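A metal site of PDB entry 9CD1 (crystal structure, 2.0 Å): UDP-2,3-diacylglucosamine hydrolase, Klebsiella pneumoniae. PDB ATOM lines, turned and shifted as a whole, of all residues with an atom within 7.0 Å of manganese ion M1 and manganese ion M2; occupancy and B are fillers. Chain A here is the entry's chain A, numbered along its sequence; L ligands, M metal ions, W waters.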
ATOM      1  N   ALA A   7     -35.225  11.530   9.459  1.00  0.00           N
ATOM      2  CA  ALA A   7     -34.300  11.405   8.338  1.00  0.00           C
ATOM      3  C   ALA A   7     -33.370  12.618   8.327  1.00  0.00           C
ATOM      4  O   ALA A   7     -33.603  13.603   9.030  1.00  0.00           O
ATOM      5  CB  ALA A   7     -35.034  11.297   6.996  1.00  0.00           C
ATOM      6  N   ASP A   8     -32.312  12.506   7.521  1.00  0.00           N
ATOM      7  CA  ASP A   8     -31.425  13.625   7.224  1.00  0.00           C
ATOM      8  C   ASP A   8     -30.804  14.211   8.490  1.00  0.00           C
ATOM      9  O   ASP A   8     -30.728  15.432   8.665  1.00  0.00           O
ATOM     10  CB  ASP A   8     -32.161  14.693   6.416  1.00  0.00           C
ATOM     11  CG  ASP A   8     -32.646  14.170   5.079  1.00  0.00           C
ATOM     12  OD1 ASP A   8     -31.796  13.865   4.219  1.00  0.00           O
ATOM     13  OD2 ASP A   8     -33.872  14.025   4.903  1.00  0.00           O
ATOM     14  N   LEU A   9     -30.346  13.332   9.384  1.00  0.00           N
ATOM     15  CA  LEU A   9     -29.599  13.780  10.555  1.00  0.00           C
ATOM     16  C   LEU A   9     -28.172  14.154  10.183  1.00  0.00           C
ATOM     17  O   LEU A   9     -27.588  15.053  10.792  1.00  0.00           O
ATOM     18  CB  LEU A   9     -29.619  12.696  11.623  1.00  0.00           C
ATOM     19  CG  LEU A   9     -30.907  12.548  12.440  1.00  0.00           C
ATOM     20  CD1 LEU A   9     -31.934  11.698  11.706  1.00  0.00           C
ATOM     21  CD2 LEU A   9     -30.583  11.943  13.796  1.00  0.00           C
ATOM     22  N   HIS A  10     -27.594  13.464   9.197  1.00  0.00           N
ATOM     23  CA  HIS A  10     -26.239  13.737   8.718  1.00  0.00           C
ATOM     24  C   HIS A  10     -25.236  13.743   9.869  1.00  0.00           C
ATOM     25  O   HIS A  10     -24.430  14.665  10.029  1.00  0.00           O
ATOM     26  CB  HIS A  10     -26.187  15.070   7.946  1.00  0.00           C
ATOM     27  CG  HIS A  10     -27.026  15.075   6.701  1.00  0.00           C
ATOM     28  ND1 HIS A  10     -26.529  14.706   5.468  1.00  0.00           N
ATOM     29  CD2 HIS A  10     -28.319  15.400   6.504  1.00  0.00           C
ATOM     30  CE1 HIS A  10     -27.485  14.804   4.565  1.00  0.00           C
ATOM     31  NE2 HIS A  10     -28.587  15.227   5.170  1.00  0.00           N
ATOM     32  N   LEU A  39     -35.499   7.262   7.536  1.00  0.00           N
ATOM     33  CA  LEU A  39     -35.632   7.289   6.082  1.00  0.00           C
ATOM     34  C   LEU A  39     -34.418   7.874   5.382  1.00  0.00           C
ATOM     35  O   LEU A  39     -34.565   8.690   4.464  1.00  0.00           O
ATOM     36  CB  LEU A  39     -36.894   8.070   5.719  1.00  0.00           C
ATOM     37  CG  LEU A  39     -38.209   7.586   6.328  1.00  0.00           C
ATOM     38  CD1 LEU A  39     -39.383   8.341   5.728  1.00  0.00           C
ATOM     39  CD2 LEU A  39     -38.373   6.082   6.140  1.00  0.00           C
ATOM     40  N   GLY A  40     -33.204   7.478   5.756  1.00  0.00           N
ATOM     41  CA  GLY A  40     -32.044   7.808   4.969  1.00  0.00           C
ATOM     42  C   GLY A  40     -31.292   9.017   5.503  1.00  0.00           C
ATOM     43  O   GLY A  40     -31.831   9.866   6.208  1.00  0.00           O
ATOM     44  N   ASP A  41     -30.010   9.085   5.119  1.00  0.00           N
ATOM     45  CA  ASP A  41     -29.112  10.159   5.535  1.00  0.00           C
ATOM     46  C   ASP A  41     -29.011  10.248   7.059  1.00  0.00           C
ATOM     47  O   ASP A  41     -28.973  11.351   7.633  1.00  0.00           O
ATOM     48  CB  ASP A  41     -29.530  11.503   4.922  1.00  0.00           C
ATOM     49  CG  ASP A  41     -29.189  11.610   3.450  1.00  0.00           C
ATOM     50  OD1 ASP A  41     -28.694  10.609   2.874  1.00  0.00           O
ATOM     51  OD2 ASP A  41     -29.426  12.679   2.866  1.00  0.00           O
ATOM     52  N   GLU A  44     -23.656  11.440   7.689  1.00  0.00           N
ATOM     53  CA  GLU A  44     -23.179  12.308   6.627  1.00  0.00           C
ATOM     54  C   GLU A  44     -22.386  11.528   5.578  1.00  0.00           C
ATOM     55  O   GLU A  44     -22.347  11.923   4.402  1.00  0.00           O
ATOM     56  CB  GLU A  44     -22.330  13.444   7.211  1.00  0.00           C
ATOM     57  CG  GLU A  44     -21.594  14.311   6.195  1.00  0.00           C
ATOM     58  CD  GLU A  44     -22.512  15.120   5.293  1.00  0.00           C
ATOM     59  OE1 GLU A  44     -23.727  15.198   5.554  1.00  0.00           O
ATOM     60  OE2 GLU A  44     -22.008  15.684   4.294  1.00  0.00           O
ATOM     61  N   GLY A  78     -30.194   6.469   2.424  1.00  0.00           N
ATOM     62  CA  GLY A  78     -30.130   7.746   1.751  1.00  0.00           C
ATOM     63  C   GLY A  78     -28.995   7.790   0.738  1.00  0.00           C
ATOM     64  O   GLY A  78     -28.286   6.813   0.512  1.00  0.00           O
ATOM     65  N   ASN A  79     -28.841   8.956   0.117  1.00  0.00           N
ATOM     66  CA  ASN A  79     -27.754   9.121  -0.840  1.00  0.00           C
ATOM     67  C   ASN A  79     -26.397   9.269  -0.149  1.00  0.00           C
ATOM     68  O   ASN A  79     -25.367   9.028  -0.794  1.00  0.00           O
ATOM     69  CB  ASN A  79     -28.002  10.323  -1.742  1.00  0.00           C
ATOM     70  CG  ASN A  79     -28.221  11.608  -0.968  1.00  0.00           C
ATOM     71  OD1 ASN A  79     -29.217  11.744  -0.252  1.00  0.00           O
ATOM     72  ND2 ASN A  79     -27.290  12.545  -1.100  1.00  0.00           N
ATOM     73  N   ARG A  80     -26.373   9.651   1.127  1.00  0.00           N
ATOM     74  CA  ARG A  80     -25.111   9.785   1.839  1.00  0.00           C
ATOM     75  C   ARG A  80     -24.636   8.449   2.411  1.00  0.00           C
ATOM     76  O   ARG A  80     -23.439   8.164   2.403  1.00  0.00           O
ATOM     77  CB  ARG A  80     -25.237  10.820   2.961  1.00  0.00           C
ATOM     78  CG  ARG A  80     -25.713  12.197   2.489  1.00  0.00           C
ATOM     79  CD  ARG A  80     -24.782  12.785   1.435  1.00  0.00           C
ATOM     80  NE  ARG A  80     -23.430  12.978   1.938  1.00  0.00           N
ATOM     81  CZ  ARG A  80     -22.486  13.667   1.305  1.00  0.00           C
ATOM     82  NH1 ARG A  80     -22.720  14.247   0.137  1.00  0.00           N
ATOM     83  NH2 ARG A  80     -21.285  13.788   1.864  1.00  0.00           N
ATOM     84  N   HIS A 114     -36.532   7.563   0.851  1.00  0.00           N
ATOM     85  CA  HIS A 114     -35.666   8.698   1.179  1.00  0.00           C
ATOM     86  C   HIS A 114     -36.101   9.949   0.440  1.00  0.00           C
ATOM     87  O   HIS A 114     -36.067  11.052   0.997  1.00  0.00           O
ATOM     88  CB  HIS A 114     -34.209   8.369   0.858  1.00  0.00           C
ATOM     89  CG  HIS A 114     -33.265   9.478   1.199  1.00  0.00           C
ATOM     90  ND1 HIS A 114     -33.154   9.994   2.479  1.00  0.00           N
ATOM     91  CD2 HIS A 114     -32.408  10.194   0.436  1.00  0.00           C
ATOM     92  CE1 HIS A 114     -32.264  10.973   2.479  1.00  0.00           C
ATOM     93  NE2 HIS A 114     -31.795  11.115   1.251  1.00  0.00           N
ATOM     94  N   GLY A 115     -36.519   9.812  -0.821  1.00  0.00           N
ATOM     95  CA  GLY A 115     -37.028  10.911  -1.607  1.00  0.00           C
ATOM     96  C   GLY A 115     -36.130  11.346  -2.741  1.00  0.00           C
ATOM     97  O   GLY A 115     -36.582  12.112  -3.605  1.00  0.00           O
ATOM     98  N   ASP A 116     -34.869  10.892  -2.783  1.00  0.00           N
ATOM     99  CA  ASP A 116     -33.980  11.332  -3.856  1.00  0.00           C
ATOM    100  C   ASP A 116     -34.405  10.774  -5.210  1.00  0.00           C
ATOM    101  O   ASP A 116     -34.136  11.406  -6.237  1.00  0.00           O
ATOM    102  CB  ASP A 116     -32.526  10.928  -3.550  1.00  0.00           C
ATOM    103  CG  ASP A 116     -32.367   9.433  -3.357  1.00  0.00           C
ATOM    104  OD1 ASP A 116     -33.089   8.856  -2.519  1.00  0.00           O
ATOM    105  OD2 ASP A 116     -31.517   8.840  -4.055  1.00  0.00           O
ATOM    106  N   TYR A 125     -27.229  14.000 -10.669  1.00  0.00           N
ATOM    107  CA  TYR A 125     -27.250  13.157  -9.485  1.00  0.00           C
ATOM    108  C   TYR A 125     -27.725  11.748  -9.821  1.00  0.00           C
ATOM    109  O   TYR A 125     -27.212  10.760  -9.273  1.00  0.00           O
ATOM    110  CB  TYR A 125     -28.152  13.751  -8.399  1.00  0.00           C
ATOM    111  CG  TYR A 125     -28.494  12.723  -7.346  1.00  0.00           C
ATOM    112  CD1 TYR A 125     -27.532  12.284  -6.446  1.00  0.00           C
ATOM    113  CD2 TYR A 125     -29.764  12.154  -7.295  1.00  0.00           C
ATOM    114  CE1 TYR A 125     -27.835  11.327  -5.496  1.00  0.00           C
ATOM    115  CE2 TYR A 125     -30.073  11.204  -6.349  1.00  0.00           C
ATOM    116  CZ  TYR A 125     -29.102  10.788  -5.451  1.00  0.00           C
ATOM    117  OH  TYR A 125     -29.405   9.839  -4.514  1.00  0.00           O
ATOM    118  N   ILE A 171     -29.613  21.231  -2.687  1.00  0.00           N
ATOM    119  CA  ILE A 171     -30.377  20.054  -3.077  1.00  0.00           C
ATOM    120  C   ILE A 171     -31.608  20.468  -3.873  1.00  0.00           C
ATOM    121  O   ILE A 171     -32.408  21.279  -3.413  1.00  0.00           O
ATOM    122  CB  ILE A 171     -30.779  19.215  -1.860  1.00  0.00           C
ATOM    123  CG1 ILE A 171     -29.556  18.913  -0.987  1.00  0.00           C
ATOM    124  CG2 ILE A 171     -31.451  17.923  -2.292  1.00  0.00           C
ATOM    125  CD1 ILE A 171     -29.904  18.421   0.397  1.00  0.00           C
ATOM    126  N   GLY A 194     -37.751  12.279   2.984  1.00  0.00           N
ATOM    127  CA  GLY A 194     -36.860  13.360   3.354  1.00  0.00           C
ATOM    128  C   GLY A 194     -36.051  13.847   2.173  1.00  0.00           C
ATOM    129  O   GLY A 194     -36.612  14.194   1.136  1.00  0.00           O
ATOM    130  N   HIS A 195     -34.722  13.885   2.346  1.00  0.00           N
ATOM    131  CA  HIS A 195     -33.750  14.243   1.310  1.00  0.00           C
ATOM    132  C   HIS A 195     -33.776  15.723   0.925  1.00  0.00           C
ATOM    133  O   HIS A 195     -32.718  16.349   0.823  1.00  0.00           O
ATOM    134  CB  HIS A 195     -33.948  13.393   0.053  1.00  0.00           C
ATOM    135  CG  HIS A 195     -33.008  13.748  -1.053  1.00  0.00           C
ATOM    136  ND1 HIS A 195     -31.657  13.483  -0.999  1.00  0.00           N
ATOM    137  CD2 HIS A 195     -33.210  14.375  -2.240  1.00  0.00           C
ATOM    138  CE1 HIS A 195     -31.074  13.917  -2.107  1.00  0.00           C
ATOM    139  NE2 HIS A 195     -31.992  14.467  -2.870  1.00  0.00           N
ATOM    140  N   THR A 196     -34.958  16.285   0.672  1.00  0.00           N
ATOM    141  CA  THR A 196     -35.023  17.655   0.166  1.00  0.00           C
ATOM    142  C   THR A 196     -34.793  18.704   1.249  1.00  0.00           C
ATOM    143  O   THR A 196     -34.559  19.870   0.907  1.00  0.00           O
ATOM    144  CB  THR A 196     -36.366  17.917  -0.522  1.00  0.00           C
ATOM    145  OG1 THR A 196     -37.427  17.748   0.419  1.00  0.00           O
ATOM    146  CG2 THR A 196     -36.556  16.967  -1.691  1.00  0.00           C
ATOM    147  N   HIS A 197     -34.860  18.325   2.525  1.00  0.00           N
ATOM    148  CA  HIS A 197     -34.599  19.242   3.644  1.00  0.00           C
ATOM    149  C   HIS A 197     -35.598  20.396   3.657  1.00  0.00           C
ATOM    150  O   HIS A 197     -35.273  21.505   4.099  1.00  0.00           O
ATOM    151  CB  HIS A 197     -33.162  19.769   3.617  1.00  0.00           C
ATOM    152  CG  HIS A 197     -32.116  18.705   3.728  1.00  0.00           C
ATOM    153  ND1 HIS A 197     -30.776  18.987   3.878  1.00  0.00           N
ATOM    154  CD2 HIS A 197     -32.210  17.350   3.736  1.00  0.00           C
ATOM    155  CE1 HIS A 197     -30.087  17.867   3.954  1.00  0.00           C
ATOM    156  NE2 HIS A 197     -30.938  16.852   3.875  1.00  0.00           N
ATOM    157  N   ALA A 218     -34.184  18.359   7.935  1.00  0.00           N
ATOM    158  CA  ALA A 218     -32.831  17.968   8.327  1.00  0.00           C
ATOM    159  C   ALA A 218     -32.531  18.486   9.726  1.00  0.00           C
ATOM    160  O   ALA A 218     -33.097  19.486  10.181  1.00  0.00           O
ATOM    161  CB  ALA A 218     -31.801  18.504   7.329  1.00  0.00           C
HETATM  162  C1  LIG L   1     -18.997   5.823  -0.788  1.00  0.00           C
HETATM  163  C2  LIG L   1     -21.890  10.017  -0.509  1.00  0.00           C
HETATM  164  C3  LIG L   1     -21.990  11.716  -2.227  1.00  0.00           C
HETATM  165  C4  LIG L   1     -24.128  12.655  -3.493  1.00  0.00           C
HETATM  166  C5  LIG L   1     -25.342  14.621  -4.720  1.00  0.00           C
HETATM  167  C6  LIG L   1     -27.459  14.877  -3.296  1.00  0.00           C
HETATM  168  C7  LIG L   1     -18.941   3.597  -4.354  1.00  0.00           C
HETATM  169  C8  LIG L   1     -18.139   5.379  -3.147  1.00  0.00           C
HETATM  170  C9  LIG L   1     -17.242   7.234  -1.585  1.00  0.00           C
HETATM  171  C10 LIG L   1     -17.956   8.454  -1.001  1.00  0.00           C
HETATM  172  C11 LIG L   1     -19.742   7.039  -0.234  1.00  0.00           C
HETATM  173  C12 LIG L   1     -20.547  10.348  -0.295  1.00  0.00           C
HETATM  174  C13 LIG L   1     -22.622  10.710  -1.490  1.00  0.00           C
HETATM  175  C14 LIG L   1     -20.647  12.012  -2.019  1.00  0.00           C
HETATM  176  C15 LIG L   1     -19.923  11.339  -1.042  1.00  0.00           C
HETATM  177  C16 LIG L   1     -24.487  13.504  -4.750  1.00  0.00           C
HETATM  178  C17 LIG L   1     -25.068  17.649  -2.497  1.00  0.00           C
HETATM  179  C18 LIG L   1     -25.583  15.321  -5.905  1.00  0.00           C
HETATM  180  C19 LIG L   1     -24.971  14.932  -7.104  1.00  0.00           C
HETATM  181  C20 LIG L   1     -24.113  13.837  -7.129  1.00  0.00           C
HETATM  182  C21 LIG L   1     -23.872  13.137  -5.944  1.00  0.00           C
HETATM  183  C22 LIG L   1     -17.161   5.630  -4.125  1.00  0.00           C
HETATM  184  C23 LIG L   1     -17.098   4.800  -5.248  1.00  0.00           C
HETATM  185  C24 LIG L   1     -18.009   3.756  -5.373  1.00  0.00           C
HETATM  186  C25 LIG L   1     -16.035   5.064  -6.338  1.00  0.00           C
HETATM  187  F1  LIG L   1     -15.806   3.907  -7.015  1.00  0.00           F
HETATM  188  F2  LIG L   1     -14.866   5.487  -5.752  1.00  0.00           F
HETATM  189  F3  LIG L   1     -16.481   6.030  -7.195  1.00  0.00           F
HETATM  190  N1  LIG L   1     -18.974   4.396  -3.289  1.00  0.00           N
HETATM  191  N2  LIG L   1     -18.233   6.225  -1.941  1.00  0.00           N
HETATM  192  N3  LIG L   1     -18.843   8.128   0.117  1.00  0.00           N
HETATM  193  N4  LIG L   1     -22.683  12.480  -3.312  1.00  0.00           N
HETATM  194  N5  LIG L   1     -25.998  15.067  -3.471  1.00  0.00           N
HETATM  195  O1  LIG L   1     -20.351   8.980   2.089  1.00  0.00           O
HETATM  196  O2  LIG L   1     -18.510  10.313   1.565  1.00  0.00           O
HETATM  197  O3  LIG L   1     -24.934  12.190  -2.756  1.00  0.00           O
HETATM  198  O4  LIG L   1     -23.674  15.331  -2.219  1.00  0.00           O
HETATM  199  O5  LIG L   1     -25.525  15.490  -0.892  1.00  0.00           O
HETATM  200  S1  LIG L   1     -19.542   9.460   0.962  1.00  0.00           S
HETATM  201  S2  LIG L   1     -25.057  15.841  -2.240  1.00  0.00           S
HETATM  202 CL1  LIG L   1     -20.138   2.276  -4.438  1.00  0.00          CL
HETATM  203 MN    MN M   1     -30.102  14.743   3.632  1.00  0.00          MN
HETATM  204 MN    MN M   2     -30.383  12.829   0.907  1.00  0.00          MN
HETATM  205  O   HOH W   1     -30.288  14.800   1.670  1.00  0.00           O
HETATM  206  O   HOH W   2     -28.052  14.787   0.784  1.00  0.00           O
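An oxygen (O3) of the ligand lies within hydrogen-bond range of the side-chain amide nitrogen (ND2) of Asn 79. NH1 of Arg 80 lies within hydrogen-bond range of O4 of the ligand (2.8 Å).
The backbone NH of Arg 80 is in hydrogen-bond range of the side-chain carboxylate of Asp 41 (3.1 Å). ND1 of His 114 lies within hydrogen-bond range of O of Leu 39, 2.8 Å away. The side-chain carboxylate (OD2) of Asp 8 is in hydrogen-bond range of the backbone NH (N) of His 195. The backbone NH (N) of Gly 194 is in hydrogen-bond range of the backbone carbonyl oxygen (O) of His 114, 2.9 Å away. The side-chain carboxylate of Glu 44 sits at hydrogen-bond distance from a ring nitrogen (ND1) of His 10. O of Gly 40 lies within hydrogen-bond range of N of Asp 8 (3.0 Å). The backbone NH of Leu 9 is in hydrogen-bond range of the backbone carbonyl oxygen of Asp 41 (3.0 Å).
Of the 21 residues printed, 4 come within 4 Å of manganese ion M1. The nearest printed residue that does not touch manganese ion M1 is His 195 (4.2 Å).
Of the 21 residues printed, 5 come within 4 Å of manganese ion M2.
Manganese ion M1 is bound by water W1 (2.0 Å), the side-chain carboxylate (OD1) of Asp 8 (2.0 Å), a ring nitrogen (NE2) of His 10 (2.2 Å), a ring nitrogen (NE2) of His 197 (2.3 Å) and the side-chain carboxylate (OD2) of Asp 41 (2.3 Å).
Manganese ion M2 is bound by OD1 of Asn 79, 2.0 Å away. Water W1 binds manganese ion M2, at 2.1 Å. Manganese ion M2 is bound by OD2 of Asp 41 (2.2 Å). A ring nitrogen (NE2) of His 114 binds manganese ion M2, at 2.2 Å. ND1 of His 195 is bound to manganese ion M2 (2.4 Å). Manganese ion M2 has five donor atoms within binding distance.
Water W2 lies within hydrogen-bond range of ND2 of Asn 79 (3.0 Å) and O5 of the ligand (3.1 Å).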
